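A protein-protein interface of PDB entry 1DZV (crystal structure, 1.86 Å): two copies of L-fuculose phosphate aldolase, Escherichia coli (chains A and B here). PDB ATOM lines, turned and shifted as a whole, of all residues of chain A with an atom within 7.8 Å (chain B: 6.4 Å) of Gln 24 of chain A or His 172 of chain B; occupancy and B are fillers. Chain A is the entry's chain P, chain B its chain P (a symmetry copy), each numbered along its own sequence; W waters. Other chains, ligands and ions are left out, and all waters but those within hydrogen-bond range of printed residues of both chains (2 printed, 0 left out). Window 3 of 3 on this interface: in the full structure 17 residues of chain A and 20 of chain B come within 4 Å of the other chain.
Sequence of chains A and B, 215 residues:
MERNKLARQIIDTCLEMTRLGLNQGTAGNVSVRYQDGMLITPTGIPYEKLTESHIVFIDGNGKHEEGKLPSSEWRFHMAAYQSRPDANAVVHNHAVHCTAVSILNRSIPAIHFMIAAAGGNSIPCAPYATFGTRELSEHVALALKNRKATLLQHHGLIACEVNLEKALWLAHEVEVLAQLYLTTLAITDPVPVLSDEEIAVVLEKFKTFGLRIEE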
ATOM      1  N   MET A  17     -27.151 -20.035  -7.171  1.00  0.00           N
ATOM      2  CA  MET A  17     -26.459 -18.789  -7.425  1.00  0.00           C
ATOM      3  C   MET A  17     -25.235 -18.653  -6.511  1.00  0.00           C
ATOM      4  O   MET A  17     -24.187 -18.186  -6.935  1.00  0.00           O
ATOM      5  CB  MET A  17     -27.286 -17.538  -7.103  1.00  0.00           C
ATOM      6  CG  MET A  17     -28.139 -17.072  -8.254  1.00  0.00           C
ATOM      7  SD  MET A  17     -28.465 -15.308  -8.191  1.00  0.00           S
ATOM      8  CE  MET A  17     -29.150 -15.119  -6.553  1.00  0.00           C
ATOM      9  N   THR A  18     -25.444 -19.045  -5.262  1.00  0.00           N
ATOM     10  CA  THR A  18     -24.386 -19.015  -4.250  1.00  0.00           C
ATOM     11  C   THR A  18     -23.363 -20.083  -4.593  1.00  0.00           C
ATOM     12  O   THR A  18     -22.160 -19.817  -4.633  1.00  0.00           O
ATOM     13  CB  THR A  18     -24.981 -19.188  -2.843  1.00  0.00           C
ATOM     14  OG1 THR A  18     -25.840 -18.061  -2.597  1.00  0.00           O
ATOM     15  CG2 THR A  18     -23.913 -19.201  -1.764  1.00  0.00           C
ATOM     16  N   GLY A  21     -20.930 -18.817  -7.324  1.00  0.00           N
ATOM     17  CA  GLY A  21     -20.087 -17.685  -7.008  1.00  0.00           C
ATOM     18  C   GLY A  21     -20.668 -16.359  -7.469  1.00  0.00           C
ATOM     19  O   GLY A  21     -19.959 -15.356  -7.529  1.00  0.00           O
ATOM     20  N   LEU A  22     -21.963 -16.347  -7.776  1.00  0.00           N
ATOM     21  CA  LEU A  22     -22.635 -15.150  -8.253  1.00  0.00           C
ATOM     22  C   LEU A  22     -23.248 -14.341  -7.117  1.00  0.00           C
ATOM     23  O   LEU A  22     -23.649 -13.195  -7.297  1.00  0.00           O
ATOM     24  CB  LEU A  22     -23.770 -15.529  -9.231  1.00  0.00           C
ATOM     25  CG  LEU A  22     -23.333 -16.323 -10.462  1.00  0.00           C
ATOM     26  CD1 LEU A  22     -24.531 -16.806 -11.263  1.00  0.00           C
ATOM     27  CD2 LEU A  22     -22.411 -15.475 -11.316  1.00  0.00           C
ATOM     28  N   ASN A  23     -23.390 -14.990  -5.978  1.00  0.00           N
ATOM     29  CA  ASN A  23     -24.052 -14.357  -4.842  1.00  0.00           C
ATOM     30  C   ASN A  23     -23.262 -14.670  -3.577  1.00  0.00           C
ATOM     31  O   ASN A  23     -22.851 -15.775  -3.233  1.00  0.00           O
ATOM     32  CB  ASN A  23     -25.510 -14.785  -4.759  1.00  0.00           C
ATOM     33  CG  ASN A  23     -26.404 -14.232  -3.685  1.00  0.00           C
ATOM     34  OD1 ASN A  23     -26.671 -13.030  -3.583  1.00  0.00           O
ATOM     35  ND2 ASN A  23     -26.937 -15.121  -2.829  1.00  0.00           N
ATOM     36  N   GLN A  24     -22.995 -13.564  -2.901  1.00  0.00           N
ATOM     37  CA  GLN A  24     -22.294 -13.542  -1.632  1.00  0.00           C
ATOM     38  C   GLN A  24     -23.266 -12.893  -0.638  1.00  0.00           C
ATOM     39  O   GLN A  24     -24.099 -12.081  -1.058  1.00  0.00           O
ATOM     40  CB  GLN A  24     -21.023 -12.699  -1.705  1.00  0.00           C
ATOM     41  CG  GLN A  24     -20.544 -12.341  -3.095  1.00  0.00           C
ATOM     42  CD  GLN A  24     -19.331 -13.115  -3.551  1.00  0.00           C
ATOM     43  OE1 GLN A  24     -18.659 -12.717  -4.509  1.00  0.00           O
ATOM     44  NE2 GLN A  24     -19.005 -14.224  -2.889  1.00  0.00           N
ATOM     45  N   GLY A  25     -23.134 -13.250   0.629  1.00  0.00           N
ATOM     46  CA  GLY A  25     -23.962 -12.645   1.660  1.00  0.00           C
ATOM     47  C   GLY A  25     -25.449 -12.685   1.333  1.00  0.00           C
ATOM     48  O   GLY A  25     -25.994 -13.678   0.842  1.00  0.00           O
ATOM     49  N   THR A  26     -26.116 -11.573   1.622  1.00  0.00           N
ATOM     50  CA  THR A  26     -27.560 -11.468   1.448  1.00  0.00           C
ATOM     51  C   THR A  26     -27.956 -10.670   0.218  1.00  0.00           C
ATOM     52  O   THR A  26     -29.125 -10.316   0.039  1.00  0.00           O
ATOM     53  CB  THR A  26     -28.130 -10.785   2.720  1.00  0.00           C
ATOM     54  OG1 THR A  26     -27.439  -9.534   2.914  1.00  0.00           O
ATOM     55  CG2 THR A  26     -27.931 -11.681   3.934  1.00  0.00           C
ATOM     56  N   ALA A  27     -27.000 -10.391  -0.661  1.00  0.00           N
ATOM     57  CA  ALA A  27     -27.197  -9.529  -1.807  1.00  0.00           C
ATOM     58  C   ALA A  27     -28.231  -9.930  -2.840  1.00  0.00           C
ATOM     59  O   ALA A  27     -28.935  -9.028  -3.318  1.00  0.00           O
ATOM     60  CB  ALA A  27     -25.825  -9.295  -2.451  1.00  0.00           C
ATOM     61  N   GLY A  28     -28.410 -11.157  -3.287  1.00  0.00           N
ATOM     62  CA  GLY A  28     -29.375 -11.385  -4.370  1.00  0.00           C
ATOM     63  C   GLY A  28     -30.846 -11.410  -4.002  1.00  0.00           C
ATOM     64  O   GLY A  28     -31.242 -11.467  -2.842  1.00  0.00           O
ATOM     65  N   TYR A  47     -30.093 -16.838   2.752  1.00  0.00           N
ATOM     66  CA  TYR A  47     -30.536 -17.852   1.812  1.00  0.00           C
ATOM     67  C   TYR A  47     -30.735 -19.244   2.396  1.00  0.00           C
ATOM     68  O   TYR A  47     -31.727 -19.919   2.106  1.00  0.00           O
ATOM     69  CB  TYR A  47     -29.573 -17.885   0.605  1.00  0.00           C
ATOM     70  CG  TYR A  47     -28.237 -18.554   0.851  1.00  0.00           C
ATOM     71  CD1 TYR A  47     -28.102 -19.923   0.652  1.00  0.00           C
ATOM     72  CD2 TYR A  47     -27.113 -17.855   1.279  1.00  0.00           C
ATOM     73  CE1 TYR A  47     -26.903 -20.576   0.875  1.00  0.00           C
ATOM     74  CE2 TYR A  47     -25.904 -18.492   1.505  1.00  0.00           C
ATOM     75  CZ  TYR A  47     -25.805 -19.854   1.301  1.00  0.00           C
ATOM     76  OH  TYR A  47     -24.616 -20.524   1.509  1.00  0.00           O
ATOM     77  N   ASN A  93     -28.349  -9.861  -8.815  1.00  0.00           N
ATOM     78  CA  ASN A  93     -27.297 -10.166  -7.821  1.00  0.00           C
ATOM     79  C   ASN A  93     -26.265  -9.067  -7.955  1.00  0.00           C
ATOM     80  O   ASN A  93     -26.396  -8.165  -8.805  1.00  0.00           O
ATOM     81  CB  ASN A  93     -26.741 -11.566  -8.064  1.00  0.00           C
ATOM     82  CG  ASN A  93     -26.124 -11.729  -9.445  1.00  0.00           C
ATOM     83  OD1 ASN A  93     -25.359 -10.869  -9.894  1.00  0.00           O
ATOM     84  ND2 ASN A  93     -26.437 -12.841 -10.130  1.00  0.00           N
ATOM     85  N   HIS A  94     -25.274  -9.116  -7.096  1.00  0.00           N
ATOM     86  CA  HIS A  94     -24.153  -8.199  -7.095  1.00  0.00           C
ATOM     87  C   HIS A  94     -22.884  -9.007  -7.435  1.00  0.00           C
ATOM     88  O   HIS A  94     -21.871  -8.901  -6.761  1.00  0.00           O
ATOM     89  CB  HIS A  94     -24.019  -7.438  -5.784  1.00  0.00           C
ATOM     90  CG  HIS A  94     -25.198  -6.667  -5.285  1.00  0.00           C
ATOM     91  ND1 HIS A  94     -25.210  -6.058  -4.049  1.00  0.00           N
ATOM     92  CD2 HIS A  94     -26.410  -6.376  -5.831  1.00  0.00           C
ATOM     93  CE1 HIS A  94     -26.378  -5.457  -3.847  1.00  0.00           C
ATOM     94  NE2 HIS A  94     -27.137  -5.638  -4.933  1.00  0.00           N
ATOM     95  N   ALA A  95     -22.913  -9.826  -8.472  1.00  0.00           N
ATOM     96  CA  ALA A  95     -21.751 -10.614  -8.906  1.00  0.00           C
ATOM     97  C   ALA A  95     -20.570  -9.673  -9.130  1.00  0.00           C
ATOM     98  O   ALA A  95     -20.691  -8.589  -9.693  1.00  0.00           O
ATOM     99  CB  ALA A  95     -22.100 -11.390 -10.166  1.00  0.00           C
ATOM    100  N   VAL A  96     -19.391 -10.093  -8.663  1.00  0.00           N
ATOM    101  CA  VAL A  96     -18.230  -9.220  -8.601  1.00  0.00           C
ATOM    102  C   VAL A  96     -17.770  -8.696  -9.944  1.00  0.00           C
ATOM    103  O   VAL A  96     -17.601  -7.450 -10.030  1.00  0.00           O
ATOM    104  CB  VAL A  96     -17.049  -9.792  -7.793  1.00  0.00           C
ATOM    105  CG1 VAL A  96     -17.498 -10.191  -6.398  1.00  0.00           C
ATOM    106  CG2 VAL A  96     -16.364 -10.944  -8.515  1.00  0.00           C
ATOM    107  N   HIS A  97     -17.636  -9.477 -11.004  1.00  0.00           N
ATOM    108  CA  HIS A  97     -17.164  -8.924 -12.281  1.00  0.00           C
ATOM    109  C   HIS A  97     -18.179  -7.985 -12.912  1.00  0.00           C
ATOM    110  O   HIS A  97     -17.857  -6.879 -13.348  1.00  0.00           O
ATOM    111  CB  HIS A  97     -16.731 -10.053 -13.244  1.00  0.00           C
ATOM    112  CG  HIS A  97     -15.612 -10.840 -12.621  1.00  0.00           C
ATOM    113  ND1 HIS A  97     -15.774 -12.050 -12.000  1.00  0.00           N
ATOM    114  CD2 HIS A  97     -14.283 -10.518 -12.523  1.00  0.00           C
ATOM    115  CE1 HIS A  97     -14.592 -12.448 -11.542  1.00  0.00           C
ATOM    116  NE2 HIS A  97     -13.663 -11.554 -11.864  1.00  0.00           N
ATOM    117  N   GLU A 175     -21.851 -12.788 -16.194  1.00  0.00           N
ATOM    118  CA  GLU A 175     -20.698 -12.681 -15.281  1.00  0.00           C
ATOM    119  C   GLU A 175     -19.462 -13.186 -16.001  1.00  0.00           C
ATOM    120  O   GLU A 175     -18.381 -12.575 -15.851  1.00  0.00           O
ATOM    121  CB  GLU A 175     -20.967 -13.464 -13.988  1.00  0.00           C
ATOM    122  CG  GLU A 175     -19.851 -13.575 -12.975  1.00  0.00           C
ATOM    123  CD  GLU A 175     -19.448 -12.243 -12.353  1.00  0.00           C
ATOM    124  OE1 GLU A 175     -19.975 -11.148 -12.695  1.00  0.00           O
ATOM    125  OE2 GLU A 175     -18.552 -12.289 -11.497  1.00  0.00           O
ATOM    126  N   LEU B  20     -15.690 -19.618   3.000  1.00  0.00           N
ATOM    127  CA  LEU B  20     -15.865 -18.449   2.164  1.00  0.00           C
ATOM    128  C   LEU B  20     -14.629 -17.927   1.451  1.00  0.00           C
ATOM    129  O   LEU B  20     -14.728 -17.001   0.640  1.00  0.00           O
ATOM    130  CB  LEU B  20     -16.480 -17.322   3.017  1.00  0.00           C
ATOM    131  CG  LEU B  20     -17.936 -17.489   3.458  1.00  0.00           C
ATOM    132  CD1 LEU B  20     -18.329 -16.397   4.457  1.00  0.00           C
ATOM    133  CD2 LEU B  20     -18.925 -17.439   2.292  1.00  0.00           C
ATOM    134  N   GLY B  21     -13.445 -18.430   1.760  1.00  0.00           N
ATOM    135  CA  GLY B  21     -12.211 -18.005   1.136  1.00  0.00           C
ATOM    136  C   GLY B  21     -11.594 -16.786   1.800  1.00  0.00           C
ATOM    137  O   GLY B  21     -10.715 -16.144   1.229  1.00  0.00           O
ATOM    138  N   LEU B  22     -12.038 -16.478   3.017  1.00  0.00           N
ATOM    139  CA  LEU B  22     -11.548 -15.323   3.751  1.00  0.00           C
ATOM    140  C   LEU B  22     -10.363 -15.668   4.645  1.00  0.00           C
ATOM    141  O   LEU B  22      -9.676 -14.789   5.157  1.00  0.00           O
ATOM    142  CB  LEU B  22     -12.666 -14.747   4.648  1.00  0.00           C
ATOM    143  CG  LEU B  22     -13.934 -14.311   3.913  1.00  0.00           C
ATOM    144  CD1 LEU B  22     -15.037 -13.935   4.888  1.00  0.00           C
ATOM    145  CD2 LEU B  22     -13.612 -13.159   2.981  1.00  0.00           C
ATOM    146  N   ASN B  93      -9.008 -11.290   9.933  1.00  0.00           N
ATOM    147  CA  ASN B  93      -8.422 -12.305   9.031  1.00  0.00           C
ATOM    148  C   ASN B  93      -7.447 -11.560   8.144  1.00  0.00           C
ATOM    149  O   ASN B  93      -7.299 -10.327   8.248  1.00  0.00           O
ATOM    150  CB  ASN B  93      -9.529 -13.022   8.264  1.00  0.00           C
ATOM    151  CG  ASN B  93     -10.366 -12.082   7.411  1.00  0.00           C
ATOM    152  OD1 ASN B  93      -9.822 -11.229   6.700  1.00  0.00           O
ATOM    153  ND2 ASN B  93     -11.700 -12.233   7.457  1.00  0.00           N
ATOM    154  N   ALA B 167     -20.918 -10.139  12.153  1.00  0.00           N
ATOM    155  CA  ALA B 167     -19.516  -9.725  12.004  1.00  0.00           C
ATOM    156  C   ALA B 167     -18.902 -10.473  10.816  1.00  0.00           C
ATOM    157  O   ALA B 167     -18.088  -9.918  10.076  1.00  0.00           O
ATOM    158  CB  ALA B 167     -18.666  -9.899  13.257  1.00  0.00           C
ATOM    159  N   LEU B 168     -19.219 -11.755  10.648  1.00  0.00           N
ATOM    160  CA  LEU B 168     -18.688 -12.484   9.487  1.00  0.00           C
ATOM    161  C   LEU B 168     -19.217 -11.888   8.190  1.00  0.00           C
ATOM    162  O   LEU B 168     -18.534 -11.779   7.156  1.00  0.00           O
ATOM    163  CB  LEU B 168     -19.035 -13.966   9.636  1.00  0.00           C
ATOM    164  CG  LEU B 168     -18.563 -14.884   8.489  1.00  0.00           C
ATOM    165  CD1 LEU B 168     -17.063 -14.769   8.255  1.00  0.00           C
ATOM    166  CD2 LEU B 168     -18.912 -16.341   8.777  1.00  0.00           C
ATOM    167  N   TRP B 169     -20.516 -11.562   8.176  1.00  0.00           N
ATOM    168  CA  TRP B 169     -21.173 -11.011   6.993  1.00  0.00           C
ATOM    169  C   TRP B 169     -20.514  -9.712   6.541  1.00  0.00           C
ATOM    170  O   TRP B 169     -20.243  -9.463   5.356  1.00  0.00           O
ATOM    171  CB  TRP B 169     -22.677 -10.827   7.290  1.00  0.00           C
ATOM    172  CG  TRP B 169     -23.362 -10.047   6.201  1.00  0.00           C
ATOM    173  CD1 TRP B 169     -23.872 -10.548   5.031  1.00  0.00           C
ATOM    174  CD2 TRP B 169     -23.562  -8.628   6.161  1.00  0.00           C
ATOM    175  NE1 TRP B 169     -24.401  -9.529   4.273  1.00  0.00           N
ATOM    176  CE2 TRP B 169     -24.216  -8.337   4.945  1.00  0.00           C
ATOM    177  CE3 TRP B 169     -23.269  -7.576   7.035  1.00  0.00           C
ATOM    178  CZ2 TRP B 169     -24.564  -7.030   4.593  1.00  0.00           C
ATOM    179  CZ3 TRP B 169     -23.613  -6.284   6.692  1.00  0.00           C
ATOM    180  CH2 TRP B 169     -24.262  -6.027   5.470  1.00  0.00           C
ATOM    181  N   LEU B 170     -20.225  -8.832   7.516  1.00  0.00           N
ATOM    182  CA  LEU B 170     -19.552  -7.587   7.228  1.00  0.00           C
ATOM    183  C   LEU B 170     -18.147  -7.841   6.662  1.00  0.00           C
ATOM    184  O   LEU B 170     -17.731  -7.150   5.736  1.00  0.00           O
ATOM    185  CB  LEU B 170     -19.392  -6.742   8.475  1.00  0.00           C
ATOM    186  CG  LEU B 170     -19.476  -5.234   8.438  1.00  0.00           C
ATOM    187  CD1 LEU B 170     -18.743  -4.666   9.644  1.00  0.00           C
ATOM    188  CD2 LEU B 170     -19.094  -4.530   7.152  1.00  0.00           C
ATOM    189  N   ALA B 171     -17.421  -8.741   7.314  1.00  0.00           N
ATOM    190  CA  ALA B 171     -16.064  -9.063   6.854  1.00  0.00           C
ATOM    191  C   ALA B 171     -16.086  -9.558   5.414  1.00  0.00           C
ATOM    192  O   ALA B 171     -15.244  -9.145   4.603  1.00  0.00           O
ATOM    193  CB  ALA B 171     -15.448 -10.111   7.775  1.00  0.00           C
ATOM    194  N   HIS B 172     -17.070 -10.409   5.074  1.00  0.00           N
ATOM    195  CA  HIS B 172     -17.183 -10.887   3.704  1.00  0.00           C
ATOM    196  C   HIS B 172     -17.526  -9.743   2.759  1.00  0.00           C
ATOM    197  O   HIS B 172     -16.884  -9.550   1.721  1.00  0.00           O
ATOM    198  CB  HIS B 172     -18.196 -12.041   3.677  1.00  0.00           C
ATOM    199  CG  HIS B 172     -18.285 -12.668   2.321  1.00  0.00           C
ATOM    200  ND1 HIS B 172     -17.212 -13.335   1.755  1.00  0.00           N
ATOM    201  CD2 HIS B 172     -19.263 -12.685   1.384  1.00  0.00           C
ATOM    202  CE1 HIS B 172     -17.538 -13.778   0.554  1.00  0.00           C
ATOM    203  NE2 HIS B 172     -18.769 -13.398   0.304  1.00  0.00           N
ATOM    204  N   GLU B 173     -18.446  -8.856   3.110  1.00  0.00           N
ATOM    205  CA  GLU B 173     -18.775  -7.685   2.308  1.00  0.00           C
ATOM    206  C   GLU B 173     -17.561  -6.764   2.070  1.00  0.00           C
ATOM    207  O   GLU B 173     -17.386  -6.192   0.981  1.00  0.00           O
ATOM    208  CB  GLU B 173     -19.890  -6.845   2.904  1.00  0.00           C
ATOM    209  CG  GLU B 173     -21.313  -7.333   2.886  1.00  0.00           C
ATOM    210  CD  GLU B 173     -21.816  -7.751   1.517  1.00  0.00           C
ATOM    211  OE1 GLU B 173     -21.821  -6.942   0.562  1.00  0.00           O
ATOM    212  OE2 GLU B 173     -22.212  -8.943   1.396  1.00  0.00           O
ATOM    213  N   VAL B 174     -16.702  -6.583   3.049  1.00  0.00           N
ATOM    214  CA  VAL B 174     -15.536  -5.720   2.862  1.00  0.00           C
ATOM    215  C   VAL B 174     -14.545  -6.370   1.901  1.00  0.00           C
ATOM    216  O   VAL B 174     -13.915  -5.686   1.084  1.00  0.00           O
ATOM    217  CB  VAL B 174     -14.881  -5.385   4.211  1.00  0.00           C
ATOM    218  CG1 VAL B 174     -13.600  -4.603   4.012  1.00  0.00           C
ATOM    219  CG2 VAL B 174     -15.874  -4.630   5.101  1.00  0.00           C
ATOM    220  N   GLU B 175     -14.399  -7.711   1.974  1.00  0.00           N
ATOM    221  CA  GLU B 175     -13.526  -8.407   1.013  1.00  0.00           C
ATOM    222  C   GLU B 175     -14.096  -8.225  -0.381  1.00  0.00           C
ATOM    223  O   GLU B 175     -13.314  -8.010  -1.332  1.00  0.00           O
ATOM    224  CB  GLU B 175     -13.396  -9.891   1.389  1.00  0.00           C
ATOM    225  CG  GLU B 175     -12.636 -10.800   0.452  1.00  0.00           C
ATOM    226  CD  GLU B 175     -11.153 -10.466   0.335  1.00  0.00           C
ATOM    227  OE1 GLU B 175     -10.629  -9.488   0.937  1.00  0.00           O
ATOM    228  OE2 GLU B 175     -10.484 -11.203  -0.405  1.00  0.00           O
ATOM    229  N   VAL B 176     -15.423  -8.308  -0.592  1.00  0.00           N
ATOM    230  CA  VAL B 176     -15.957  -8.005  -1.919  1.00  0.00           C
ATOM    231  C   VAL B 176     -15.687  -6.574  -2.385  1.00  0.00           C
ATOM    232  O   VAL B 176     -15.308  -6.313  -3.546  1.00  0.00           O
ATOM    233  CB  VAL B 176     -17.484  -8.294  -1.996  1.00  0.00           C
ATOM    234  CG1 VAL B 176     -18.068  -7.818  -3.307  1.00  0.00           C
ATOM    235  CG2 VAL B 176     -17.687  -9.799  -1.845  1.00  0.00           C
ATOM    236  N   LEU B 177     -15.899  -5.578  -1.527  1.00  0.00           N
ATOM    237  CA  LEU B 177     -15.573  -4.193  -1.879  1.00  0.00           C
ATOM    238  C   LEU B 177     -14.093  -4.022  -2.229  1.00  0.00           C
ATOM    239  O   LEU B 177     -13.695  -3.328  -3.171  1.00  0.00           O
ATOM    240  CB  LEU B 177     -15.900  -3.293  -0.675  1.00  0.00           C
ATOM    241  CG  LEU B 177     -17.374  -2.990  -0.423  1.00  0.00           C
ATOM    242  CD1 LEU B 177     -17.612  -2.293   0.918  1.00  0.00           C
ATOM    243  CD2 LEU B 177     -17.951  -2.164  -1.577  1.00  0.00           C
ATOM    244  N   GLN B 179     -12.023  -6.335  -3.501  1.00  0.00           N
ATOM    245  CA  GLN B 179     -11.890  -6.966  -4.790  1.00  0.00           C
ATOM    246  C   GLN B 179     -12.444  -6.057  -5.882  1.00  0.00           C
ATOM    247  O   GLN B 179     -11.789  -5.894  -6.898  1.00  0.00           O
ATOM    248  CB  GLN B 179     -12.615  -8.312  -4.865  1.00  0.00           C
ATOM    249  CG  GLN B 179     -12.142  -9.073  -6.109  1.00  0.00           C
ATOM    250  CD  GLN B 179     -12.818 -10.423  -6.270  1.00  0.00           C
ATOM    251  OE1 GLN B 179     -13.471 -10.881  -5.336  1.00  0.00           O
ATOM    252  NE2 GLN B 179     -12.663 -11.025  -7.450  1.00  0.00           N
HETATM  253  O   HOH W   1     -24.893  -8.040   0.767  1.00  0.00           O
HETATM  254  O   HOH W   2     -23.231  -6.282  -2.334  1.00  0.00           O
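The side-chain amide nitrogen of Gln 24 of chain A sits close to a ring nitrogen (NE2) of His 172 of chain B, 3.3 Å away.
OG1 of Thr 26 of chain A is in hydrogen-bond range of NE1 of Trp 169 of chain B (3.3 Å).
Among the printed residues, merely in contact across the chains: Gly 25 of chain A with Trp 169 of chain B, Gly 25 of chain A with His 172 of chain B, Val 96 of chain A with Val 176 of chain B and Val 96 of chain A with Gln 179 of chain B.
Of the printed residues of chain B, Gln 24 of chain A touches His 172.
Of the printed residues of chain A, His 172 of chain B touches Gln 24 and Gly 25.
No residue of chain A comes within 4 Å of Ala 171 of chain B.
Of the printed residues of chain A, Trp 169 of chain B touches Gly 25 (3.97 Å) and Thr 26 (3.3 Å).
Of the printed residues of chain B, Thr 26 of chain A touches Trp 169 (3.3 Å).
Of the printed residues of chain A, Val 176 of chain B touches Val 96 (3.9 Å).
Printed residues of chain B within 4 Å of Gly 25 of chain A: Trp 169 (3.97 Å) and His 172 (3.98 Å).
Of the printed residues of chain A, Gln 179 of chain B touches Val 96.
Leu 170 of chain B touches none of the printed residues of chain A.
The nearest residue of chain B that does not touch Gln 24 of chain A is Val 176 of chain B (4.02 Å).
Among the printed residues, no Asp or Glu carboxylate lies within 4 Å of a Lys or Arg side-chain nitrogen of the other chain.
Positions printed for both chains: 21, 22, 93 and 175.
Of the 6 pairs that touch across the chains among the printed residues, none has its exchanged pair printed and touching as well.
Water W2 bridges a ring nitrogen (ND1) of His 94 of chain A (2.6 Å) and the side-chain carboxylate (OE1) of Glu 173 of chain B (3.3 Å).
Water W1 bridges the side-chain carboxylate of Glu 173 of chain B (2.9 Å) and the backbone NH of Ala 27 of chain A (3.5 Å).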
